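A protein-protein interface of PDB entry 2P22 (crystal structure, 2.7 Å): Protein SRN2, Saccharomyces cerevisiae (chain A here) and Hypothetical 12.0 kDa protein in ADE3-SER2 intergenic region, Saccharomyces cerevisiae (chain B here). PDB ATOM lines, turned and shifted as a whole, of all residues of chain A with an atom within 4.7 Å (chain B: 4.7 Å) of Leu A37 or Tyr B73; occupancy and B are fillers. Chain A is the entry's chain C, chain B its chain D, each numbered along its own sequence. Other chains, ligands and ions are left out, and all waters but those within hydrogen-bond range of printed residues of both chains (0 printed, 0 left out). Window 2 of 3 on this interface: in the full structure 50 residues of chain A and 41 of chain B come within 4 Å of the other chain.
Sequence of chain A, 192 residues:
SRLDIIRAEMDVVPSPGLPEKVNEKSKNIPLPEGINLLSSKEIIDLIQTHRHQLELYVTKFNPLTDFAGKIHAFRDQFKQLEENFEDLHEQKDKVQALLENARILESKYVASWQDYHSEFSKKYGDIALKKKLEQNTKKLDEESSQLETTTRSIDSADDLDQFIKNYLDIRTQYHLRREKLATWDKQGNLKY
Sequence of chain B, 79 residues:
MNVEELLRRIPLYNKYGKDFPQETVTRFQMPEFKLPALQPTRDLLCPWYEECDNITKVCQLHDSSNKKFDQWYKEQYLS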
ATOM      1  N   PRO A  32     -14.116  11.839  -0.364  1.00  0.00           N
ATOM      2  CA  PRO A  32     -15.507  12.214  -0.672  1.00  0.00           C
ATOM      3  C   PRO A  32     -15.999  11.434  -1.910  1.00  0.00           C
ATOM      4  O   PRO A  32     -16.566  10.365  -1.758  1.00  0.00           O
ATOM      5  CB  PRO A  32     -15.405  13.723  -0.905  1.00  0.00           C
ATOM      6  CG  PRO A  32     -14.284  14.124   0.027  1.00  0.00           C
ATOM      7  CD  PRO A  32     -13.266  13.033  -0.205  1.00  0.00           C
ATOM      8  N   GLU A  33     -15.786  11.981  -3.116  1.00  0.00           N
ATOM      9  CA  GLU A  33     -16.145  11.347  -4.412  1.00  0.00           C
ATOM     10  C   GLU A  33     -15.163  11.853  -5.487  1.00  0.00           C
ATOM     11  O   GLU A  33     -15.487  11.929  -6.689  1.00  0.00           O
ATOM     12  CB  GLU A  33     -17.577  11.687  -4.848  1.00  0.00           C
ATOM     13  CG  GLU A  33     -18.664  11.058  -4.007  1.00  0.00           C
ATOM     14  CD  GLU A  33     -18.728  11.640  -2.605  1.00  0.00           C
ATOM     15  OE1 GLU A  33     -18.592  12.871  -2.484  1.00  0.00           O
ATOM     16  OE2 GLU A  33     -18.914  10.880  -1.628  1.00  0.00           O
ATOM     17  N   GLY A  34     -13.960  12.188  -5.016  1.00  0.00           N
ATOM     18  CA  GLY A  34     -12.897  12.710  -5.858  1.00  0.00           C
ATOM     19  C   GLY A  34     -12.829  12.143  -7.264  1.00  0.00           C
ATOM     20  O   GLY A  34     -12.447  12.842  -8.199  1.00  0.00           O
ATOM     21  N   ILE A  35     -13.214  10.885  -7.434  1.00  0.00           N
ATOM     22  CA  ILE A  35     -13.154  10.280  -8.755  1.00  0.00           C
ATOM     23  C   ILE A  35     -13.917  11.065  -9.816  1.00  0.00           C
ATOM     24  O   ILE A  35     -13.597  11.002 -10.996  1.00  0.00           O
ATOM     25  CB  ILE A  35     -13.689   8.854  -8.745  1.00  0.00           C
ATOM     26  CG1 ILE A  35     -13.110   8.082  -7.564  1.00  0.00           C
ATOM     27  CG2 ILE A  35     -13.265   8.160 -10.024  1.00  0.00           C
ATOM     28  CD1 ILE A  35     -11.652   7.750  -7.733  1.00  0.00           C
ATOM     29  N   ASN A  36     -14.924  11.817  -9.406  1.00  0.00           N
ATOM     30  CA  ASN A  36     -15.687  12.584 -10.375  1.00  0.00           C
ATOM     31  C   ASN A  36     -15.100  13.962 -10.668  1.00  0.00           C
ATOM     32  O   ASN A  36     -15.422  14.569 -11.696  1.00  0.00           O
ATOM     33  CB  ASN A  36     -17.132  12.737  -9.904  1.00  0.00           C
ATOM     34  CG  ASN A  36     -18.090  11.799 -10.630  1.00  0.00           C
ATOM     35  OD1 ASN A  36     -19.262  11.688 -10.261  1.00  0.00           O
ATOM     36  ND2 ASN A  36     -17.596  11.128 -11.676  1.00  0.00           N
ATOM     37  N   LEU A  37     -14.245  14.458  -9.774  1.00  0.00           N
ATOM     38  CA  LEU A  37     -13.635  15.770  -9.970  1.00  0.00           C
ATOM     39  C   LEU A  37     -12.713  15.829 -11.183  1.00  0.00           C
ATOM     40  O   LEU A  37     -12.016  14.858 -11.509  1.00  0.00           O
ATOM     41  CB  LEU A  37     -12.873  16.218  -8.718  1.00  0.00           C
ATOM     42  CG  LEU A  37     -13.596  17.293  -7.905  1.00  0.00           C
ATOM     43  CD1 LEU A  37     -14.803  16.685  -7.204  1.00  0.00           C
ATOM     44  CD2 LEU A  37     -12.636  17.886  -6.906  1.00  0.00           C
ATOM     45  N   LEU A  38     -12.720  17.000 -11.822  1.00  0.00           N
ATOM     46  CA  LEU A  38     -11.955  17.289 -13.031  1.00  0.00           C
ATOM     47  C   LEU A  38     -10.626  16.579 -13.102  1.00  0.00           C
ATOM     48  O   LEU A  38      -9.978  16.329 -12.078  1.00  0.00           O
ATOM     49  CB  LEU A  38     -11.749  18.802 -13.191  1.00  0.00           C
ATOM     50  CG  LEU A  38     -11.998  19.412 -14.584  1.00  0.00           C
ATOM     51  CD1 LEU A  38     -13.426  19.120 -15.060  1.00  0.00           C
ATOM     52  CD2 LEU A  38     -11.764  20.919 -14.527  1.00  0.00           C
ATOM     53  N   SER A  39     -10.246  16.256 -14.337  1.00  0.00           N
ATOM     54  CA  SER A  39      -9.004  15.557 -14.647  1.00  0.00           C
ATOM     55  C   SER A  39      -7.899  15.890 -13.634  1.00  0.00           C
ATOM     56  O   SER A  39      -6.968  15.103 -13.426  1.00  0.00           O
ATOM     57  CB  SER A  39      -8.559  15.913 -16.078  1.00  0.00           C
ATOM     58  OG  SER A  39      -7.443  15.137 -16.489  1.00  0.00           O
ATOM     59  N   GLU A  42      -9.735  20.433 -10.768  1.00  0.00           N
ATOM     60  CA  GLU A  42     -10.648  20.547  -9.639  1.00  0.00           C
ATOM     61  C   GLU A  42     -10.039  19.948  -8.362  1.00  0.00           C
ATOM     62  O   GLU A  42     -10.198  20.499  -7.269  1.00  0.00           O
ATOM     63  CB  GLU A  42     -11.990  19.891  -9.981  1.00  0.00           C
ATOM     64  CG  GLU A  42     -12.839  20.735 -10.929  1.00  0.00           C
ATOM     65  CD  GLU A  42     -14.181  20.090 -11.283  1.00  0.00           C
ATOM     66  OE1 GLU A  42     -14.183  18.959 -11.822  1.00  0.00           O
ATOM     67  OE2 GLU A  42     -15.236  20.717 -11.028  1.00  0.00           O
ATOM     68  N   ILE A  43      -9.329  18.833  -8.509  1.00  0.00           N
ATOM     69  CA  ILE A  43      -8.672  18.186  -7.379  1.00  0.00           C
ATOM     70  C   ILE A  43      -7.603  19.137  -6.847  1.00  0.00           C
ATOM     71  O   ILE A  43      -7.525  19.405  -5.640  1.00  0.00           O
ATOM     72  CB  ILE A  43      -8.042  16.870  -7.836  1.00  0.00           C
ATOM     73  CG1 ILE A  43      -9.169  15.883  -8.169  1.00  0.00           C
ATOM     74  CG2 ILE A  43      -7.120  16.316  -6.775  1.00  0.00           C
ATOM     75  CD1 ILE A  43      -8.687  14.550  -8.650  1.00  0.00           C
ATOM     76  N   LEU A  46      -9.103  21.947  -5.287  1.00  0.00           N
ATOM     77  CA  LEU A  46      -9.647  21.526  -4.009  1.00  0.00           C
ATOM     78  C   LEU A  46      -8.546  21.429  -2.960  1.00  0.00           C
ATOM     79  O   LEU A  46      -8.738  21.865  -1.836  1.00  0.00           O
ATOM     80  CB  LEU A  46     -10.387  20.194  -4.183  1.00  0.00           C
ATOM     81  CG  LEU A  46     -11.183  19.502  -3.065  1.00  0.00           C
ATOM     82  CD1 LEU A  46     -10.343  18.387  -2.496  1.00  0.00           C
ATOM     83  CD2 LEU A  46     -11.631  20.480  -1.992  1.00  0.00           C
ATOM     84  N   PHE B  69     -19.159  20.790   5.128  1.00  0.00           N
ATOM     85  CA  PHE B  69     -18.297  20.491   3.988  1.00  0.00           C
ATOM     86  C   PHE B  69     -19.087  19.949   2.791  1.00  0.00           C
ATOM     87  O   PHE B  69     -18.880  20.369   1.655  1.00  0.00           O
ATOM     88  CB  PHE B  69     -17.230  19.473   4.397  1.00  0.00           C
ATOM     89  CG  PHE B  69     -16.439  18.940   3.248  1.00  0.00           C
ATOM     90  CD1 PHE B  69     -15.516  19.738   2.596  1.00  0.00           C
ATOM     91  CD2 PHE B  69     -16.651  17.649   2.786  1.00  0.00           C
ATOM     92  CE1 PHE B  69     -14.816  19.259   1.490  1.00  0.00           C
ATOM     93  CE2 PHE B  69     -15.953  17.157   1.677  1.00  0.00           C
ATOM     94  CZ  PHE B  69     -15.037  17.963   1.029  1.00  0.00           C
ATOM     95  N   ASP B  70     -19.988  19.007   3.056  1.00  0.00           N
ATOM     96  CA  ASP B  70     -20.793  18.423   2.000  1.00  0.00           C
ATOM     97  C   ASP B  70     -21.620  19.466   1.285  1.00  0.00           C
ATOM     98  O   ASP B  70     -21.740  19.409   0.072  1.00  0.00           O
ATOM     99  CB  ASP B  70     -21.708  17.335   2.554  1.00  0.00           C
ATOM    100  CG  ASP B  70     -21.012  16.001   2.670  1.00  0.00           C
ATOM    101  OD1 ASP B  70     -20.460  15.531   1.651  1.00  0.00           O
ATOM    102  OD2 ASP B  70     -21.016  15.417   3.773  1.00  0.00           O
ATOM    103  N   GLN B  71     -22.194  20.410   2.026  1.00  0.00           N
ATOM    104  CA  GLN B  71     -22.995  21.459   1.408  1.00  0.00           C
ATOM    105  C   GLN B  71     -22.098  22.215   0.428  1.00  0.00           C
ATOM    106  O   GLN B  71     -22.449  22.384  -0.736  1.00  0.00           O
ATOM    107  CB  GLN B  71     -23.548  22.414   2.471  1.00  0.00           C
ATOM    108  CG  GLN B  71     -24.200  21.698   3.661  1.00  0.00           C
ATOM    109  CD  GLN B  71     -24.663  22.653   4.774  1.00  0.00           C
ATOM    110  OE1 GLN B  71     -23.920  23.541   5.200  1.00  0.00           O
ATOM    111  NE2 GLN B  71     -25.890  22.451   5.257  1.00  0.00           N
ATOM    112  N   TRP B  72     -20.927  22.642   0.900  1.00  0.00           N
ATOM    113  CA  TRP B  72     -19.962  23.367   0.076  1.00  0.00           C
ATOM    114  C   TRP B  72     -19.486  22.503  -1.088  1.00  0.00           C
ATOM    115  O   TRP B  72     -19.427  22.957  -2.227  1.00  0.00           O
ATOM    116  CB  TRP B  72     -18.739  23.795   0.915  1.00  0.00           C
ATOM    117  CG  TRP B  72     -17.612  24.334   0.067  1.00  0.00           C
ATOM    118  CD1 TRP B  72     -17.543  25.567  -0.516  1.00  0.00           C
ATOM    119  CD2 TRP B  72     -16.501  23.588  -0.453  1.00  0.00           C
ATOM    120  NE1 TRP B  72     -16.469  25.630  -1.380  1.00  0.00           N
ATOM    121  CE2 TRP B  72     -15.814  24.429  -1.359  1.00  0.00           C
ATOM    122  CE3 TRP B  72     -16.026  22.288  -0.245  1.00  0.00           C
ATOM    123  CZ2 TRP B  72     -14.681  24.010  -2.060  1.00  0.00           C
ATOM    124  CZ3 TRP B  72     -14.907  21.866  -0.935  1.00  0.00           C
ATOM    125  CH2 TRP B  72     -14.240  22.727  -1.838  1.00  0.00           C
ATOM    126  N   TYR B  73     -19.137  21.260  -0.780  1.00  0.00           N
ATOM    127  CA  TYR B  73     -18.655  20.298  -1.765  1.00  0.00           C
ATOM    128  C   TYR B  73     -19.669  20.053  -2.882  1.00  0.00           C
ATOM    129  O   TYR B  73     -19.296  19.701  -3.996  1.00  0.00           O
ATOM    130  CB  TYR B  73     -18.328  18.982  -1.057  1.00  0.00           C
ATOM    131  CG  TYR B  73     -17.816  17.881  -1.957  1.00  0.00           C
ATOM    132  CD1 TYR B  73     -16.542  17.948  -2.529  1.00  0.00           C
ATOM    133  CD2 TYR B  73     -18.579  16.740  -2.181  1.00  0.00           C
ATOM    134  CE1 TYR B  73     -16.039  16.892  -3.294  1.00  0.00           C
ATOM    135  CE2 TYR B  73     -18.092  15.688  -2.938  1.00  0.00           C
ATOM    136  CZ  TYR B  73     -16.824  15.759  -3.486  1.00  0.00           C
ATOM    137  OH  TYR B  73     -16.342  14.664  -4.161  1.00  0.00           O
ATOM    138  N   LYS B  74     -20.948  20.223  -2.569  1.00  0.00           N
ATOM    139  CA  LYS B  74     -22.014  20.048  -3.546  1.00  0.00           C
ATOM    140  C   LYS B  74     -21.979  21.188  -4.571  1.00  0.00           C
ATOM    141  O   LYS B  74     -21.627  20.966  -5.724  1.00  0.00           O
ATOM    142  CB  LYS B  74     -23.378  20.027  -2.844  1.00  0.00           C
ATOM    143  CG  LYS B  74     -24.583  20.175  -3.782  1.00  0.00           C
ATOM    144  CD  LYS B  74     -25.918  20.228  -3.031  1.00  0.00           C
ATOM    145  CE  LYS B  74     -27.097  20.360  -3.998  1.00  0.00           C
ATOM    146  NZ  LYS B  74     -28.430  20.269  -3.328  1.00  0.00           N
ATOM    147  N   GLU B  75     -22.337  22.400  -4.146  1.00  0.00           N
ATOM    148  CA  GLU B  75     -22.346  23.565  -5.038  1.00  0.00           C
ATOM    149  C   GLU B  75     -21.061  23.645  -5.863  1.00  0.00           C
ATOM    150  O   GLU B  75     -21.077  24.091  -7.006  1.00  0.00           O
ATOM    151  CB  GLU B  75     -22.531  24.860  -4.222  1.00  0.00           C
ATOM    152  CG  GLU B  75     -22.432  26.195  -5.009  1.00  0.00           C
ATOM    153  CD  GLU B  75     -23.634  26.485  -5.911  1.00  0.00           C
ATOM    154  OE1 GLU B  75     -24.783  26.404  -5.425  1.00  0.00           O
ATOM    155  OE2 GLU B  75     -23.426  26.818  -7.102  1.00  0.00           O
ATOM    156  N   GLN B  76     -19.953  23.195  -5.288  1.00  0.00           N
ATOM    157  CA  GLN B  76     -18.677  23.236  -5.985  1.00  0.00           C
ATOM    158  C   GLN B  76     -18.498  22.207  -7.099  1.00  0.00           C
ATOM    159  O   GLN B  76     -18.040  22.551  -8.183  1.00  0.00           O
ATOM    160  CB  GLN B  76     -17.535  23.098  -4.983  1.00  0.00           C
ATOM    161  CG  GLN B  76     -17.188  24.387  -4.257  1.00  0.00           C
ATOM    162  CD  GLN B  76     -16.231  25.272  -5.037  1.00  0.00           C
ATOM    163  OE1 GLN B  76     -15.214  24.805  -5.547  1.00  0.00           O
ATOM    164  NE2 GLN B  76     -16.542  26.560  -5.113  1.00  0.00           N
ATOM    165  N   TYR B  77     -18.848  20.949  -6.846  1.00  0.00           N
ATOM    166  CA  TYR B  77     -18.690  19.914  -7.866  1.00  0.00           C
ATOM    167  C   TYR B  77     -19.953  19.053  -8.053  1.00  0.00           C
ATOM    168  O   TYR B  77     -19.920  17.836  -7.861  1.00  0.00           O
ATOM    169  CB  TYR B  77     -17.490  19.016  -7.512  1.00  0.00           C
ATOM    170  CG  TYR B  77     -16.276  19.765  -6.981  1.00  0.00           C
ATOM    171  CD1 TYR B  77     -16.110  19.990  -5.612  1.00  0.00           C
ATOM    172  CD2 TYR B  77     -15.314  20.281  -7.848  1.00  0.00           C
ATOM    173  CE1 TYR B  77     -15.011  20.716  -5.122  1.00  0.00           C
ATOM    174  CE2 TYR B  77     -14.216  21.009  -7.369  1.00  0.00           C
ATOM    175  CZ  TYR B  77     -14.071  21.224  -6.008  1.00  0.00           C
ATOM    176  OH  TYR B  77     -13.004  21.963  -5.547  1.00  0.00           O
ATOM    177  N   LEU B  78     -21.059  19.693  -8.432  1.00  0.00           N
ATOM    178  CA  LEU B  78     -22.339  19.011  -8.651  1.00  0.00           C
ATOM    179  C   LEU B  78     -23.326  19.958  -9.315  1.00  0.00           C
ATOM    180  O   LEU B  78     -22.952  21.021  -9.809  1.00  0.00           O
ATOM    181  CB  LEU B  78     -22.955  18.555  -7.329  1.00  0.00           C
ATOM    182  CG  LEU B  78     -22.374  17.381  -6.545  1.00  0.00           C
ATOM    183  CD1 LEU B  78     -23.165  17.221  -5.251  1.00  0.00           C
ATOM    184  CD2 LEU B  78     -22.447  16.106  -7.373  1.00  0.00           C
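N of Leu A38 lies within hydrogen-bond range of OE1 of Glu A42, at 2.4 Å.
Of the 11 printed residues of chain A, 6 touch a printed residue of chain B.
Hydrophobic or aromatic side chains of chain A that line the printed part of chain B: Pro A32, Leu A37 and Leu A46.
Along chain B the printed residues that touch a printed residue of chain A span positions 69 to 77.
The backbone NH (N) of Glu A33 lies within hydrogen-bond range of the side-chain hydroxyl (OH) of Tyr B73 (2.9 Å).
Pro A32 touches Phe B69.
Tyr B73 touches Pro A32 (OH to CB, 3.5 Å).
N of Gly A34 touches OH of Tyr B73, at 3.5 Å.
OH of Tyr B73 touches CD1 of Leu A37, 3.96 Å away.
CD1 of Leu A37 touches CG of Tyr B77, 3.4 Å away.
Glu A42 touches Tyr B77 (OE2 to CD2, 3.2 Å).
Trp B72 touches Leu A46.
Tyr B77 touches Leu A46 (OH to CB, 3.4 Å).
Printed residues of chain B within 4 Å of Gly A34: Tyr B73 (3.5 Å).
Of chain B, only Tyr B73 (3.96 Å) and Tyr B77 (3.4 Å) come within 4 Å of Leu A37.
Of the printed residues of chain A, Trp B72 touches Leu A46.
Tyr B73 touches four residues of chain A.
Lys B74 touches none of the printed residues of chain A.
Printed residues of chain A within 4 Å of Tyr B77: Leu A37, Glu A42 and Leu A46.
The nearest printed residue of chain B that does not touch Leu A37 is Gln B76 (6.6 Å).
The nearest printed residue of chain A that does not touch Tyr B73 is Leu A46 (5.5 Å).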
